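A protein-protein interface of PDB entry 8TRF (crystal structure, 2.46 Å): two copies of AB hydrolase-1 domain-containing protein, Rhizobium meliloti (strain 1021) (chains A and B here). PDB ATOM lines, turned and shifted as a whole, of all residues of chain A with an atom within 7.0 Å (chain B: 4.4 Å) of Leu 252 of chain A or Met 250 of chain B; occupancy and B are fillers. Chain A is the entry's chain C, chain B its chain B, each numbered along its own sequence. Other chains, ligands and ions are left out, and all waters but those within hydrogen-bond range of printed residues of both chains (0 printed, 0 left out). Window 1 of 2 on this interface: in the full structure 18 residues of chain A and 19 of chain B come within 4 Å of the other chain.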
ATOM      1  N   HIS A 221     -24.564   9.808   3.276  1.00  0.00           N
ATOM      2  CA  HIS A 221     -24.533   8.564   2.548  1.00  0.00           C
ATOM      3  C   HIS A 221     -23.332   7.743   2.994  1.00  0.00           C
ATOM      4  O   HIS A 221     -22.241   8.229   2.985  1.00  0.00           O
ATOM      5  CB  HIS A 221     -24.487   8.792   1.062  1.00  0.00           C
ATOM      6  CG  HIS A 221     -24.935   7.611   0.287  1.00  0.00           C
ATOM      7  ND1 HIS A 221     -26.167   7.535  -0.295  1.00  0.00           N
ATOM      8  CD2 HIS A 221     -24.333   6.432   0.049  1.00  0.00           C
ATOM      9  CE1 HIS A 221     -26.299   6.368  -0.878  1.00  0.00           C
ATOM     10  NE2 HIS A 221     -25.202   5.677  -0.677  1.00  0.00           N
ATOM     11  N   ILE A 222     -23.556   6.495   3.377  1.00  0.00           N
ATOM     12  CA  ILE A 222     -22.518   5.587   3.856  1.00  0.00           C
ATOM     13  C   ILE A 222     -22.357   4.463   2.843  1.00  0.00           C
ATOM     14  O   ILE A 222     -23.347   3.859   2.405  1.00  0.00           O
ATOM     15  CB  ILE A 222     -22.859   5.023   5.245  1.00  0.00           C
ATOM     16  CG1 ILE A 222     -23.000   6.162   6.262  1.00  0.00           C
ATOM     17  CG2 ILE A 222     -21.798   4.011   5.686  1.00  0.00           C
ATOM     18  CD1 ILE A 222     -23.570   5.743   7.609  1.00  0.00           C
ATOM     19  N   LEU A 223     -21.112   4.172   2.478  1.00  0.00           N
ATOM     20  CA  LEU A 223     -20.785   3.023   1.643  1.00  0.00           C
ATOM     21  C   LEU A 223     -19.979   2.042   2.479  1.00  0.00           C
ATOM     22  O   LEU A 223     -19.004   2.429   3.132  1.00  0.00           O
ATOM     23  CB  LEU A 223     -19.998   3.444   0.398  1.00  0.00           C
ATOM     24  CG  LEU A 223     -20.823   4.170  -0.666  1.00  0.00           C
ATOM     25  CD1 LEU A 223     -20.232   5.546  -0.923  1.00  0.00           C
ATOM     26  CD2 LEU A 223     -20.901   3.363  -1.955  1.00  0.00           C
ATOM     27  N   GLN A 224     -20.391   0.780   2.467  1.00  0.00           N
ATOM     28  CA  GLN A 224     -19.802  -0.202   3.359  1.00  0.00           C
ATOM     29  C   GLN A 224     -19.851  -1.564   2.689  1.00  0.00           C
ATOM     30  O   GLN A 224     -20.817  -1.888   1.991  1.00  0.00           O
ATOM     31  CB  GLN A 224     -20.535  -0.225   4.708  1.00  0.00           C
ATOM     32  CG  GLN A 224     -20.044  -1.293   5.665  1.00  0.00           C
ATOM     33  CD  GLN A 224     -18.614  -1.062   6.106  1.00  0.00           C
ATOM     34  OE1 GLN A 224     -18.213   0.067   6.390  1.00  0.00           O
ATOM     35  NE2 GLN A 224     -17.836  -2.137   6.169  1.00  0.00           N
ATOM     36  N   GLY A 225     -18.796  -2.343   2.890  1.00  0.00           N
ATOM     37  CA  GLY A 225     -18.716  -3.693   2.363  1.00  0.00           C
ATOM     38  C   GLY A 225     -18.937  -4.687   3.488  1.00  0.00           C
ATOM     39  O   GLY A 225     -18.423  -4.515   4.595  1.00  0.00           O
ATOM     40  N   MET A 226     -19.726  -5.722   3.199  1.00  0.00           N
ATOM     41  CA  MET A 226     -20.003  -6.714   4.230  1.00  0.00           C
ATOM     42  C   MET A 226     -18.790  -7.594   4.497  1.00  0.00           C
ATOM     43  O   MET A 226     -18.648  -8.134   5.600  1.00  0.00           O
ATOM     44  CB  MET A 226     -21.212  -7.558   3.837  1.00  0.00           C
ATOM     45  CG  MET A 226     -22.512  -6.775   3.815  1.00  0.00           C
ATOM     46  SD  MET A 226     -23.986  -7.821   3.870  1.00  0.00           S
ATOM     47  CE  MET A 226     -23.468  -9.110   4.991  1.00  0.00           C
ATOM     48  N   TYR A 233     -18.923  -4.380   9.256  1.00  0.00           N
ATOM     49  CA  TYR A 233     -20.015  -3.577   8.723  1.00  0.00           C
ATOM     50  C   TYR A 233     -21.023  -3.199   9.800  1.00  0.00           C
ATOM     51  O   TYR A 233     -21.726  -2.193   9.644  1.00  0.00           O
ATOM     52  CB  TYR A 233     -20.685  -4.311   7.559  1.00  0.00           C
ATOM     53  CG  TYR A 233     -21.554  -5.487   7.939  1.00  0.00           C
ATOM     54  CD1 TYR A 233     -21.021  -6.767   8.056  1.00  0.00           C
ATOM     55  CD2 TYR A 233     -22.915  -5.324   8.148  1.00  0.00           C
ATOM     56  CE1 TYR A 233     -21.825  -7.847   8.390  1.00  0.00           C
ATOM     57  CE2 TYR A 233     -23.722  -6.392   8.482  1.00  0.00           C
ATOM     58  CZ  TYR A 233     -23.177  -7.647   8.602  1.00  0.00           C
ATOM     59  OH  TYR A 233     -24.006  -8.694   8.937  1.00  0.00           O
ATOM     60  N   THR A 234     -21.086  -3.955  10.901  1.00  0.00           N
ATOM     61  CA  THR A 234     -21.958  -3.569  12.008  1.00  0.00           C
ATOM     62  C   THR A 234     -21.493  -2.274  12.665  1.00  0.00           C
ATOM     63  O   THR A 234     -22.311  -1.545  13.236  1.00  0.00           O
ATOM     64  CB  THR A 234     -22.039  -4.690  13.050  1.00  0.00           C
ATOM     65  OG1 THR A 234     -20.719  -5.152  13.369  1.00  0.00           O
ATOM     66  CG2 THR A 234     -22.853  -5.856  12.512  1.00  0.00           C
ATOM     67  N   ALA A 236     -20.342   0.341  11.001  1.00  0.00           N
ATOM     68  CA  ALA A 236     -21.039   1.337  10.193  1.00  0.00           C
ATOM     69  C   ALA A 236     -22.519   1.400  10.551  1.00  0.00           C
ATOM     70  O   ALA A 236     -23.108   2.487  10.591  1.00  0.00           O
ATOM     71  CB  ALA A 236     -20.856   1.028   8.705  1.00  0.00           C
ATOM     72  N   LEU A 237     -23.140   0.246  10.810  1.00  0.00           N
ATOM     73  CA  LEU A 237     -24.542   0.247  11.208  1.00  0.00           C
ATOM     74  C   LEU A 237     -24.729   0.941  12.550  1.00  0.00           C
ATOM     75  O   LEU A 237     -25.686   1.702  12.736  1.00  0.00           O
ATOM     76  CB  LEU A 237     -25.080  -1.183  11.264  1.00  0.00           C
ATOM     77  CG  LEU A 237     -25.093  -1.934   9.932  1.00  0.00           C
ATOM     78  CD1 LEU A 237     -25.349  -3.413  10.153  1.00  0.00           C
ATOM     79  CD2 LEU A 237     -26.125  -1.342   8.994  1.00  0.00           C
ATOM     80  N   VAL A 249     -28.564   7.470   4.376  1.00  0.00           N
ATOM     81  CA  VAL A 249     -28.729   6.275   3.560  1.00  0.00           C
ATOM     82  C   VAL A 249     -27.413   5.512   3.565  1.00  0.00           C
ATOM     83  O   VAL A 249     -26.333   6.115   3.600  1.00  0.00           O
ATOM     84  CB  VAL A 249     -29.169   6.622   2.119  1.00  0.00           C
ATOM     85  CG1 VAL A 249     -29.513   5.365   1.340  1.00  0.00           C
ATOM     86  CG2 VAL A 249     -30.373   7.563   2.154  1.00  0.00           C
ATOM     87  N   MET A 250     -27.502   4.186   3.565  1.00  0.00           N
ATOM     88  CA  MET A 250     -26.328   3.330   3.471  1.00  0.00           C
ATOM     89  C   MET A 250     -26.450   2.433   2.254  1.00  0.00           C
ATOM     90  O   MET A 250     -27.510   1.840   2.015  1.00  0.00           O
ATOM     91  CB  MET A 250     -26.146   2.471   4.721  1.00  0.00           C
ATOM     92  CG  MET A 250     -24.804   1.759   4.743  1.00  0.00           C
ATOM     93  SD  MET A 250     -24.770   0.330   5.820  1.00  0.00           S
ATOM     94  CE  MET A 250     -24.094   1.116   7.271  1.00  0.00           C
ATOM     95  N   THR A 251     -25.369   2.327   1.494  1.00  0.00           N
ATOM     96  CA  THR A 251     -25.256   1.335   0.434  1.00  0.00           C
ATOM     97  C   THR A 251     -24.383   0.207   0.971  1.00  0.00           C
ATOM     98  O   THR A 251     -23.169   0.377   1.125  1.00  0.00           O
ATOM     99  CB  THR A 251     -24.660   1.939  -0.836  1.00  0.00           C
ATOM    100  OG1 THR A 251     -25.582   2.883  -1.394  1.00  0.00           O
ATOM    101  CG2 THR A 251     -24.393   0.847  -1.864  1.00  0.00           C
ATOM    102  N   LEU A 252     -24.999  -0.931   1.278  1.00  0.00           N
ATOM    103  CA  LEU A 252     -24.284  -2.077   1.826  1.00  0.00           C
ATOM    104  C   LEU A 252     -23.928  -3.026   0.685  1.00  0.00           C
ATOM    105  O   LEU A 252     -24.821  -3.597   0.048  1.00  0.00           O
ATOM    106  CB  LEU A 252     -25.125  -2.786   2.888  1.00  0.00           C
ATOM    107  CG  LEU A 252     -24.310  -3.639   3.861  1.00  0.00           C
ATOM    108  CD1 LEU A 252     -23.161  -2.826   4.447  1.00  0.00           C
ATOM    109  CD2 LEU A 252     -25.187  -4.227   4.960  1.00  0.00           C
ATOM    110  N   ILE A 253     -22.628  -3.206   0.441  1.00  0.00           N
ATOM    111  CA  ILE A 253     -22.128  -4.062  -0.632  1.00  0.00           C
ATOM    112  C   ILE A 253     -21.767  -5.420  -0.046  1.00  0.00           C
ATOM    113  O   ILE A 253     -20.946  -5.510   0.877  1.00  0.00           O
ATOM    114  CB  ILE A 253     -20.915  -3.430  -1.337  1.00  0.00           C
ATOM    115  CG1 ILE A 253     -21.180  -1.944  -1.610  1.00  0.00           C
ATOM    116  CG2 ILE A 253     -20.590  -4.193  -2.630  1.00  0.00           C
ATOM    117  CD1 ILE A 253     -20.032  -1.191  -2.268  1.00  0.00           C
ATOM    118  N   ARG A 254     -22.363  -6.480  -0.596  1.00  0.00           N
ATOM    119  CA  ARG A 254     -22.215  -7.814  -0.020  1.00  0.00           C
ATOM    120  C   ARG A 254     -20.786  -8.336  -0.136  1.00  0.00           C
ATOM    121  O   ARG A 254     -20.268  -8.946   0.808  1.00  0.00           O
ATOM    122  CB  ARG A 254     -23.185  -8.776  -0.701  1.00  0.00           C
ATOM    123  CG  ARG A 254     -22.967 -10.231  -0.364  1.00  0.00           C
ATOM    124  CD  ARG A 254     -23.282 -10.511   1.084  1.00  0.00           C
ATOM    125  NE  ARG A 254     -23.003 -11.897   1.433  1.00  0.00           N
ATOM    126  CZ  ARG A 254     -21.787 -12.383   1.639  1.00  0.00           C
ATOM    127  NH1 ARG A 254     -20.712 -11.617   1.542  1.00  0.00           N
ATOM    128  NH2 ARG A 254     -21.648 -13.666   1.956  1.00  0.00           N
ATOM    129  N   ASP A 255     -20.140  -8.124  -1.286  1.00  0.00           N
ATOM    130  CA  ASP A 255     -18.818  -8.677  -1.556  1.00  0.00           C
ATOM    131  C   ASP A 255     -17.708  -7.640  -1.441  1.00  0.00           C
ATOM    132  O   ASP A 255     -16.573  -7.920  -1.841  1.00  0.00           O
ATOM    133  CB  ASP A 255     -18.782  -9.334  -2.944  1.00  0.00           C
ATOM    134  CG  ASP A 255     -18.923  -8.332  -4.097  1.00  0.00           C
ATOM    135  OD1 ASP A 255     -19.151  -7.125  -3.858  1.00  0.00           O
ATOM    136  OD2 ASP A 255     -18.814  -8.771  -5.264  1.00  0.00           O
ATOM    137  N   LYS A 268     -20.481   3.072  -7.468  1.00  0.00           N
ATOM    138  CA  LYS A 268     -21.457   3.409  -6.442  1.00  0.00           C
ATOM    139  C   LYS A 268     -21.050   4.663  -5.682  1.00  0.00           C
ATOM    140  O   LYS A 268     -21.914   5.464  -5.309  1.00  0.00           O
ATOM    141  CB  LYS A 268     -21.641   2.224  -5.498  1.00  0.00           C
ATOM    142  CG  LYS A 268     -22.008   0.940  -6.231  1.00  0.00           C
ATOM    143  CD  LYS A 268     -22.222  -0.221  -5.274  1.00  0.00           C
ATOM    144  CE  LYS A 268     -22.761  -1.446  -5.996  1.00  0.00           C
ATOM    145  NZ  LYS A 268     -21.924  -1.862  -7.161  1.00  0.00           N
ATOM    146  N   ILE B 222     -31.653  -4.678  -2.554  1.00  0.00           N
ATOM    147  CA  ILE B 222     -32.563  -4.720  -1.417  1.00  0.00           C
ATOM    148  C   ILE B 222     -32.816  -3.295  -0.944  1.00  0.00           C
ATOM    149  O   ILE B 222     -31.867  -2.532  -0.723  1.00  0.00           O
ATOM    150  CB  ILE B 222     -31.992  -5.574  -0.268  1.00  0.00           C
ATOM    151  CG1 ILE B 222     -31.884  -7.046  -0.679  1.00  0.00           C
ATOM    152  CG2 ILE B 222     -32.841  -5.420   0.993  1.00  0.00           C
ATOM    153  CD1 ILE B 222     -31.228  -7.918   0.373  1.00  0.00           C
ATOM    154  N   GLN B 224     -34.490  -1.391   2.267  1.00  0.00           N
ATOM    155  CA  GLN B 224     -34.849  -1.670   3.649  1.00  0.00           C
ATOM    156  C   GLN B 224     -34.833  -0.373   4.444  1.00  0.00           C
ATOM    157  O   GLN B 224     -33.958   0.473   4.244  1.00  0.00           O
ATOM    158  CB  GLN B 224     -33.879  -2.691   4.266  1.00  0.00           C
ATOM    159  CG  GLN B 224     -34.099  -2.987   5.736  1.00  0.00           C
ATOM    160  CD  GLN B 224     -35.453  -3.596   6.013  1.00  0.00           C
ATOM    161  OE1 GLN B 224     -35.952  -4.407   5.235  1.00  0.00           O
ATOM    162  NE2 GLN B 224     -36.063  -3.201   7.127  1.00  0.00           N
ATOM    163  N   ALA B 236     -32.924  -8.477   7.140  1.00  0.00           N
ATOM    164  CA  ALA B 236     -32.422  -8.374   5.783  1.00  0.00           C
ATOM    165  C   ALA B 236     -30.901  -8.455   5.720  1.00  0.00           C
ATOM    166  O   ALA B 236     -30.358  -8.847   4.682  1.00  0.00           O
ATOM    167  CB  ALA B 236     -32.935  -7.083   5.151  1.00  0.00           C
ATOM    168  N   LEU B 237     -30.197  -8.117   6.804  1.00  0.00           N
ATOM    169  CA  LEU B 237     -28.768  -8.413   6.851  1.00  0.00           C
ATOM    170  C   LEU B 237     -28.529  -9.916   6.876  1.00  0.00           C
ATOM    171  O   LEU B 237     -27.638 -10.420   6.182  1.00  0.00           O
ATOM    172  CB  LEU B 237     -28.123  -7.768   8.072  1.00  0.00           C
ATOM    173  CG  LEU B 237     -28.420  -6.290   8.263  1.00  0.00           C
ATOM    174  CD1 LEU B 237     -27.913  -5.868   9.625  1.00  0.00           C
ATOM    175  CD2 LEU B 237     -27.793  -5.473   7.155  1.00  0.00           C
ATOM    176  N   MET B 240     -28.751 -11.253   3.471  1.00  0.00           N
ATOM    177  CA  MET B 240     -27.590 -10.977   2.630  1.00  0.00           C
ATOM    178  C   MET B 240     -26.421 -11.892   2.970  1.00  0.00           C
ATOM    179  O   MET B 240     -25.656 -12.285   2.081  1.00  0.00           O
ATOM    180  CB  MET B 240     -27.182  -9.516   2.768  1.00  0.00           C
ATOM    181  CG  MET B 240     -28.125  -8.560   2.070  1.00  0.00           C
ATOM    182  SD  MET B 240     -27.627  -6.851   2.294  1.00  0.00           S
ATOM    183  CE  MET B 240     -26.198  -6.765   1.200  1.00  0.00           C
ATOM    184  N   VAL B 248     -24.865  -8.300  -4.597  1.00  0.00           N
ATOM    185  CA  VAL B 248     -26.009  -8.165  -3.713  1.00  0.00           C
ATOM    186  C   VAL B 248     -25.806  -6.843  -2.986  1.00  0.00           C
ATOM    187  O   VAL B 248     -24.824  -6.679  -2.252  1.00  0.00           O
ATOM    188  CB  VAL B 248     -26.137  -9.336  -2.731  1.00  0.00           C
ATOM    189  CG1 VAL B 248     -27.383  -9.172  -1.882  1.00  0.00           C
ATOM    190  CG2 VAL B 248     -26.173 -10.656  -3.486  1.00  0.00           C
ATOM    191  N   VAL B 249     -26.697  -5.886  -3.224  1.00  0.00           N
ATOM    192  CA  VAL B 249     -26.571  -4.539  -2.679  1.00  0.00           C
ATOM    193  C   VAL B 249     -27.840  -4.204  -1.911  1.00  0.00           C
ATOM    194  O   VAL B 249     -28.938  -4.612  -2.306  1.00  0.00           O
ATOM    195  CB  VAL B 249     -26.320  -3.500  -3.791  1.00  0.00           C
ATOM    196  CG1 VAL B 249     -26.136  -2.114  -3.193  1.00  0.00           C
ATOM    197  CG2 VAL B 249     -25.105  -3.892  -4.625  1.00  0.00           C
ATOM    198  N   MET B 250     -27.691  -3.460  -0.814  1.00  0.00           N
ATOM    199  CA  MET B 250     -28.824  -3.007  -0.018  1.00  0.00           C
ATOM    200  C   MET B 250     -28.771  -1.498   0.164  1.00  0.00           C
ATOM    201  O   MET B 250     -27.729  -0.950   0.538  1.00  0.00           O
ATOM    202  CB  MET B 250     -28.849  -3.673   1.355  1.00  0.00           C
ATOM    203  CG  MET B 250     -30.043  -3.247   2.204  1.00  0.00           C
ATOM    204  SD  MET B 250     -29.749  -3.412   3.961  1.00  0.00           S
ATOM    205  CE  MET B 250     -30.600  -4.924   4.255  1.00  0.00           C
ATOM    206  N   THR B 251     -29.903  -0.836  -0.092  1.00  0.00           N
ATOM    207  CA  THR B 251     -30.091   0.572   0.238  1.00  0.00           C
ATOM    208  C   THR B 251     -30.838   0.606   1.564  1.00  0.00           C
ATOM    209  O   THR B 251     -32.014   0.232   1.634  1.00  0.00           O
ATOM    210  CB  THR B 251     -30.855   1.317  -0.856  1.00  0.00           C
ATOM    211  OG1 THR B 251     -30.024   1.456  -2.012  1.00  0.00           O
ATOM    212  CG2 THR B 251     -31.247   2.717  -0.381  1.00  0.00           C
ATOM    213  N   LEU B 252     -30.141   1.013   2.614  1.00  0.00           N
ATOM    214  CA  LEU B 252     -30.703   1.103   3.951  1.00  0.00           C
ATOM    215  C   LEU B 252     -31.124   2.547   4.197  1.00  0.00           C
ATOM    216  O   LEU B 252     -30.288   3.458   4.151  1.00  0.00           O
ATOM    217  CB  LEU B 252     -29.684   0.638   4.989  1.00  0.00           C
ATOM    218  CG  LEU B 252     -30.221   0.439   6.406  1.00  0.00           C
ATOM    219  CD1 LEU B 252     -31.591  -0.232   6.388  1.00  0.00           C
ATOM    220  CD2 LEU B 252     -29.229  -0.352   7.252  1.00  0.00           C
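Leu 237 of chain A touches its own counterpart, Leu 237 of chain B.
Met 250 of chain B touches its own counterpart, Met 250 of chain A.
Met 250 of chain A touches Thr 251 of chain B, and with the chains exchanged Thr 251 of chain A touches Met 250 of chain B.
Met 250 of chain A touches Leu 252 of chain B, and with the chains exchanged Leu 252 of chain A touches Met 250 of chain B.
8 positions are printed for both chains.
Of the 19 pairs that touch across the chains among the printed residues, 12 have their exchanged pair printed and touching as well.
Printed residues of chain A that touch a printed residue of chain B: Met 226, Leu 237, Val 249, Met 250, Thr 251, Leu 252, Ile 253, Arg 254 and Lys 268.
Hydrophobic or aromatic side chains of chain A within 4 Å of the printed part of chain B: Met 226, Leu 237, Val 249, Met 250 and Leu 252.
Printed residues of chain B that touch a printed residue of chain A: Leu 237, Met 240, Val 248, Val 249, Met 250, Thr 251 and Leu 252.
Hydrophobic or aromatic side chains of chain B that line the printed part of chain A: Leu 237, Met 240, Val 248, Val 249 and Leu 252.
Among the printed residues, 19 pairs touch across the chains.
Among the printed residues, no Asp or Glu carboxylate lies within 4 Å of a Lys or Arg side-chain nitrogen of the other chain.
Leu 237 of chain A touches Leu 237 of chain B (CD1 to CD1, 3.6 Å).
Thr 251 of chain B touches Val 249 of chain A.
O of Leu 252 of chain B touches CA of Val 249 of chain A, 3.3 Å away.
Thr 251 of chain A touches Val 249 of chain B.
Thr 251 of chain A touches Met 250 of chain B (CA to O, 3.4 Å).
Leu 252 of chain A touches Leu 237 of chain B (CD2 to CD2, 3.6 Å).
Met 240 of chain B touches Leu 252 of chain A.
O of Val 248 of chain B touches O of Leu 252 of chain A, 3.8 Å away.
C of Ile 253 of chain A touches O of Val 248 of chain B, at 3.97 Å.
Val 249 of chain B touches Lys 268 of chain A.
N of Gln 224 of chain B lies within hydrogen-bond range of O of Thr 251 of chain B, 3.0 Å away.
NE2 of His 221 of chain A sits at hydrogen-bond distance from OG1 of Thr 251 of chain A, 2.9 Å away.
The backbone NH (N) of Thr 251 of chain A lies within hydrogen-bond range of the backbone carbonyl oxygen (O) of Ile 222 of chain A.
The backbone NH (N) of Gln 224 of chain A is in hydrogen-bond range of the backbone carbonyl oxygen (O) of Thr 251 of chain A, 3.1 Å away.
O of Gln 224 of chain A lies within hydrogen-bond range of N of Ile 253 of chain A, 2.7 Å away.
The backbone carbonyl oxygen (O) of Ile 253 of chain A sits at hydrogen-bond distance from the backbone NH (N) of Met 226 of chain A (2.6 Å).
Printed residues of chain B within 4 Å of Thr 251 of chain A: Val 249 and Met 250.
Leu 252 of chain A touches just these residues of chain B: Leu 237 (3.6 Å), Met 240 (3.6 Å), Val 248 (3.8 Å), Val 249 (3.4 Å) and Met 250 (2.8 Å).
Of the printed residues of chain B, Lys 268 of chain A touches Val 249 (3.7 Å).
Of the printed residues of chain A, Met 240 of chain B touches Met 226, Leu 252 and Arg 254.
NE of Arg 254 of chain A lies within hydrogen-bond range of O of Met 240 of chain B, at 2.8 Å.
The backbone carbonyl oxygen (O) of Val 248 of chain B lies within hydrogen-bond range of the backbone NH (N) of Arg 254 of chain A, 3.0 Å away.
N of Leu 252 of chain A sits at hydrogen-bond distance from O of Met 250 of chain B (2.8 Å).
The backbone NH (N) of Leu 252 of chain B sits at hydrogen-bond distance from the backbone carbonyl oxygen (O) of Met 250 of chain A (2.8 Å).
The backbone carbonyl oxygen of Met 250 of chain B sits close to the backbone carbonyl oxygen of Met 250 of chain A, 3.2 Å away.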
